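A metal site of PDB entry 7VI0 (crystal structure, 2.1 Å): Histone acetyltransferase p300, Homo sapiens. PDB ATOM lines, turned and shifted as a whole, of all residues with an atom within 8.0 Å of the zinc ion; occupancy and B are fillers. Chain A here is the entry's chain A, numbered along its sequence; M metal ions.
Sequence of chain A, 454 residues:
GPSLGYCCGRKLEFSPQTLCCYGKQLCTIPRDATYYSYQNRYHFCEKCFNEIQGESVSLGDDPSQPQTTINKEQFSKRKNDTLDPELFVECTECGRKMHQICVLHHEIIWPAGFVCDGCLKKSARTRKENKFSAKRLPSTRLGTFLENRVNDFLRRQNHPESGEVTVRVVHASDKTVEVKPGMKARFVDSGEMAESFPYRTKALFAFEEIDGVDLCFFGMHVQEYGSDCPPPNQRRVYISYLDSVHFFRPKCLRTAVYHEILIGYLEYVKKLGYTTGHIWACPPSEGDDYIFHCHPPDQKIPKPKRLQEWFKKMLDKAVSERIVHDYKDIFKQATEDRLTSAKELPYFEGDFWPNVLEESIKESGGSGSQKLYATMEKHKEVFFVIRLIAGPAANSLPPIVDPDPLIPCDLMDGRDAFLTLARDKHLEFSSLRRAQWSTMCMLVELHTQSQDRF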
ATOM      1  N   GLU A  90      -6.103  18.106  -0.823  1.00  0.00           N
ATOM      2  CA  GLU A  90      -7.172  18.824  -1.503  1.00  0.00           C
ATOM      3  C   GLU A  90      -7.005  18.648  -2.999  1.00  0.00           C
ATOM      4  O   GLU A  90      -5.906  18.849  -3.534  1.00  0.00           O
ATOM      5  CB  GLU A  90      -7.152  20.303  -1.122  1.00  0.00           C
ATOM      6  CG  GLU A  90      -8.422  21.062  -1.446  1.00  0.00           C
ATOM      7  CD  GLU A  90      -8.353  22.505  -1.001  1.00  0.00           C
ATOM      8  OE1 GLU A  90      -7.780  22.758   0.087  1.00  0.00           O
ATOM      9  OE2 GLU A  90      -8.857  23.382  -1.723  1.00  0.00           O
ATOM     10  N   CYS A  91      -8.078  18.255  -3.679  1.00  0.00           N
ATOM     11  CA  CYS A  91      -8.039  18.169  -5.127  1.00  0.00           C
ATOM     12  C   CYS A  91      -7.876  19.556  -5.722  1.00  0.00           C
ATOM     13  O   CYS A  91      -8.655  20.471  -5.413  1.00  0.00           O
ATOM     14  CB  CYS A  91      -9.295  17.504  -5.686  1.00  0.00           C
ATOM     15  SG  CYS A  91      -9.294  17.352  -7.495  1.00  0.00           S
ATOM     16  N   THR A  92      -6.878  19.727  -6.589  1.00  0.00           N
ATOM     17  CA  THR A  92      -6.603  21.029  -7.168  1.00  0.00           C
ATOM     18  C   THR A  92      -7.683  21.501  -8.120  1.00  0.00           C
ATOM     19  O   THR A  92      -7.575  22.619  -8.644  1.00  0.00           O
ATOM     20  CB  THR A  92      -5.248  21.007  -7.883  1.00  0.00           C
ATOM     21  OG1 THR A  92      -5.234  19.932  -8.836  1.00  0.00           O
ATOM     22  CG2 THR A  92      -4.124  20.797  -6.875  1.00  0.00           C
ATOM     23  N   GLU A  93      -8.710  20.694  -8.397  1.00  0.00           N
ATOM     24  CA  GLU A  93      -9.778  21.091  -9.301  1.00  0.00           C
ATOM     25  C   GLU A  93     -11.122  21.279  -8.607  1.00  0.00           C
ATOM     26  O   GLU A  93     -11.706  22.364  -8.692  1.00  0.00           O
ATOM     27  CB  GLU A  93      -9.882  20.063 -10.444  1.00  0.00           C
ATOM     28  CG  GLU A  93      -8.871  20.332 -11.548  1.00  0.00           C
ATOM     29  CD  GLU A  93      -8.716  19.173 -12.500  1.00  0.00           C
ATOM     30  OE1 GLU A  93      -9.718  18.491 -12.788  1.00  0.00           O
ATOM     31  OE2 GLU A  93      -7.582  18.940 -12.970  1.00  0.00           O
ATOM     32  N   CYS A  94     -11.632  20.265  -7.896  1.00  0.00           N
ATOM     33  CA  CYS A  94     -12.896  20.449  -7.203  1.00  0.00           C
ATOM     34  C   CYS A  94     -12.736  21.058  -5.824  1.00  0.00           C
ATOM     35  O   CYS A  94     -13.690  21.682  -5.324  1.00  0.00           O
ATOM     36  CB  CYS A  94     -13.654  19.113  -7.093  1.00  0.00           C
ATOM     37  SG  CYS A  94     -12.724  17.716  -6.467  1.00  0.00           S
ATOM     38  N   GLY A  95     -11.575  20.913  -5.193  1.00  0.00           N
ATOM     39  CA  GLY A  95     -11.412  21.310  -3.811  1.00  0.00           C
ATOM     40  C   GLY A  95     -11.806  20.251  -2.815  1.00  0.00           C
ATOM     41  O   GLY A  95     -11.825  20.543  -1.611  1.00  0.00           O
ATOM     42  N   ARG A  96     -12.145  19.049  -3.268  1.00  0.00           N
ATOM     43  CA  ARG A  96     -12.502  17.965  -2.362  1.00  0.00           C
ATOM     44  C   ARG A  96     -11.328  17.611  -1.458  1.00  0.00           C
ATOM     45  O   ARG A  96     -10.186  17.487  -1.912  1.00  0.00           O
ATOM     46  CB  ARG A  96     -12.952  16.732  -3.145  1.00  0.00           C
ATOM     47  N   LYS A  97     -11.621  17.439  -0.174  1.00  0.00           N
ATOM     48  CA  LYS A  97     -10.629  17.045   0.813  1.00  0.00           C
ATOM     49  C   LYS A  97     -10.744  15.556   1.060  1.00  0.00           C
ATOM     50  O   LYS A  97     -11.838  15.058   1.350  1.00  0.00           O
ATOM     51  CB  LYS A  97     -10.807  17.826   2.118  1.00  0.00           C
ATOM     52  CG  LYS A  97      -9.969  19.102   2.195  1.00  0.00           C
ATOM     53  CD  LYS A  97     -10.154  19.798   3.544  1.00  0.00           C
ATOM     54  CE  LYS A  97     -10.156  21.312   3.397  1.00  0.00           C
ATOM     55  NZ  LYS A  97     -11.124  21.965   4.315  1.00  0.00           N
ATOM     56  N   MET A  98      -9.633  14.839   0.927  1.00  0.00           N
ATOM     57  CA  MET A  98      -9.584  13.413   1.166  1.00  0.00           C
ATOM     58  C   MET A  98      -8.403  13.074   2.065  1.00  0.00           C
ATOM     59  O   MET A  98      -7.384  13.768   2.043  1.00  0.00           O
ATOM     60  CB  MET A  98      -9.445  12.610  -0.147  1.00  0.00           C
ATOM     61  CG  MET A  98      -9.975  13.312  -1.378  1.00  0.00           C
ATOM     62  SD  MET A  98     -11.660  12.820  -1.752  1.00  0.00           S
ATOM     63  CE  MET A  98     -11.383  11.408  -2.812  1.00  0.00           C
ATOM     64  N   PHE A 114      -2.426  17.062  -6.428  1.00  0.00           N
ATOM     65  CA  PHE A 114      -3.405  15.994  -6.304  1.00  0.00           C
ATOM     66  C   PHE A 114      -4.630  16.306  -7.144  1.00  0.00           C
ATOM     67  O   PHE A 114      -5.246  17.378  -6.998  1.00  0.00           O
ATOM     68  CB  PHE A 114      -3.813  15.782  -4.852  1.00  0.00           C
ATOM     69  CG  PHE A 114      -5.001  14.887  -4.691  1.00  0.00           C
ATOM     70  CD1 PHE A 114      -4.951  13.567  -5.115  1.00  0.00           C
ATOM     71  CD2 PHE A 114      -6.188  15.366  -4.150  1.00  0.00           C
ATOM     72  CE1 PHE A 114      -6.037  12.739  -4.974  1.00  0.00           C
ATOM     73  CE2 PHE A 114      -7.284  14.536  -4.009  1.00  0.00           C
ATOM     74  CZ  PHE A 114      -7.213  13.223  -4.421  1.00  0.00           C
ATOM     75  N   VAL A 115      -4.989  15.378  -8.016  1.00  0.00           N
ATOM     76  CA  VAL A 115      -6.222  15.440  -8.792  1.00  0.00           C
ATOM     77  C   VAL A 115      -7.024  14.190  -8.461  1.00  0.00           C
ATOM     78  O   VAL A 115      -6.537  13.067  -8.654  1.00  0.00           O
ATOM     79  CB  VAL A 115      -5.959  15.560 -10.302  1.00  0.00           C
ATOM     80  CG1 VAL A 115      -7.257  15.772 -11.062  1.00  0.00           C
ATOM     81  CG2 VAL A 115      -4.977  16.694 -10.574  1.00  0.00           C
ATOM     82  N   CYS A 116      -8.252  14.371  -7.974  1.00  0.00           N
ATOM     83  CA  CYS A 116      -9.051  13.256  -7.516  1.00  0.00           C
ATOM     84  C   CYS A 116      -9.519  12.394  -8.686  1.00  0.00           C
ATOM     85  O   CYS A 116      -9.467  12.807  -9.853  1.00  0.00           O
ATOM     86  CB  CYS A 116     -10.251  13.757  -6.704  1.00  0.00           C
ATOM     87  SG  CYS A 116     -11.664  14.291  -7.702  1.00  0.00           S
ATOM     88  N   ASP A 117      -9.984  11.186  -8.365  1.00  0.00           N
ATOM     89  CA  ASP A 117     -10.447  10.265  -9.396  1.00  0.00           C
ATOM     90  C   ASP A 117     -11.661  10.817 -10.129  1.00  0.00           C
ATOM     91  O   ASP A 117     -11.801  10.585 -11.335  1.00  0.00           O
ATOM     92  CB  ASP A 117     -10.793   8.914  -8.765  1.00  0.00           C
ATOM     93  CG  ASP A 117      -9.564   8.131  -8.345  1.00  0.00           C
ATOM     94  OD1 ASP A 117      -8.507   8.286  -8.984  1.00  0.00           O
ATOM     95  OD2 ASP A 117      -9.669   7.353  -7.375  1.00  0.00           O
ATOM     96  N   GLY A 118     -12.533  11.544  -9.439  1.00  0.00           N
ATOM     97  CA  GLY A 118     -13.711  12.094 -10.086  1.00  0.00           C
ATOM     98  C   GLY A 118     -13.365  13.058 -11.202  1.00  0.00           C
ATOM     99  O   GLY A 118     -13.898  12.974 -12.312  1.00  0.00           O
ATOM    100  N   CYS A 119     -12.465  14.010 -10.928  1.00  0.00           N
ATOM    101  CA  CYS A 119     -12.061  14.959 -11.955  1.00  0.00           C
ATOM    102  C   CYS A 119     -11.305  14.272 -13.074  1.00  0.00           C
ATOM    103  O   CYS A 119     -11.357  14.726 -14.225  1.00  0.00           O
ATOM    104  CB  CYS A 119     -11.194  16.060 -11.330  1.00  0.00           C
ATOM    105  SG  CYS A 119     -12.085  17.147 -10.191  1.00  0.00           S
ATOM    106  N   LEU A 120     -10.604  13.174 -12.778  1.00  0.00           N
ATOM    107  CA  LEU A 120      -9.859  12.464 -13.803  1.00  0.00           C
ATOM    108  C   LEU A 120     -10.803  11.738 -14.769  1.00  0.00           C
ATOM    109  O   LEU A 120     -10.602  11.783 -15.987  1.00  0.00           O
ATOM    110  CB  LEU A 120      -8.884  11.473 -13.167  1.00  0.00           C
ATOM    111  CG  LEU A 120      -7.580  12.063 -12.612  1.00  0.00           C
ATOM    112  CD1 LEU A 120      -6.706  10.973 -11.997  1.00  0.00           C
ATOM    113  CD2 LEU A 120      -6.814  12.809 -13.704  1.00  0.00           C
ATOM    114  N   ARG A 125      -9.026  11.119 -18.176  1.00  0.00           N
ATOM    115  CA  ARG A 125      -7.624  11.178 -17.797  1.00  0.00           C
ATOM    116  C   ARG A 125      -7.299  10.133 -16.739  1.00  0.00           C
ATOM    117  O   ARG A 125      -8.172   9.666 -16.006  1.00  0.00           O
ATOM    118  CB  ARG A 125      -7.258  12.560 -17.252  1.00  0.00           C
ATOM    119  CG  ARG A 125      -6.694  13.535 -18.263  1.00  0.00           C
ATOM    120  CD  ARG A 125      -6.542  14.900 -17.618  1.00  0.00           C
ATOM    121  NE  ARG A 125      -7.686  15.200 -16.756  1.00  0.00           N
ATOM    122  CZ  ARG A 125      -7.638  15.912 -15.640  1.00  0.00           C
ATOM    123  NH1 ARG A 125      -6.505  16.429 -15.199  1.00  0.00           N
ATOM    124  NH2 ARG A 125      -8.753  16.121 -14.953  1.00  0.00           N
HETATM  125 ZN    ZN M   1     -11.413  16.578  -8.035  1.00  0.00          ZN
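Along chain A the residues within 4 Å of the zinc ion span positions 91 to 119. The nearest printed residue that does not touch the zinc ion is Glu 93 (4.5 Å).
The zinc ion is bound by the side-chain sulfur (SG) of Cys 91, 2.3 Å away. The side-chain sulfur (SG) of Cys 116 is bound to the zinc ion, at 2.3 Å. The zinc ion is bound by the side-chain sulfur (SG) of Cys 119, at 2.3 Å. The zinc ion is bound by SG of Cys 94 (2.3 Å). The zinc ion has four donor atoms within binding distance.
O of Cys 119 is in hydrogen-bond range of NH2 of Arg 125 (3.0 Å). The backbone NH of Gly 118 sits close to the side-chain sulfur of Cys 116, at 3.4 Å. The side-chain sulfur of Cys 91 lies close to the backbone NH of Glu 93, 3.5 Å away. The backbone NH (N) of Cys 91 lies within hydrogen-bond range of the backbone carbonyl oxygen (O) of Arg 96. The side-chain sulfur of Cys 94 sits close to the backbone NH of Arg 96. The side-chain sulfur (SG) of Cys 119 sits close to the side-chain carboxylate (OE1) of Glu 93 (3.8 Å).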
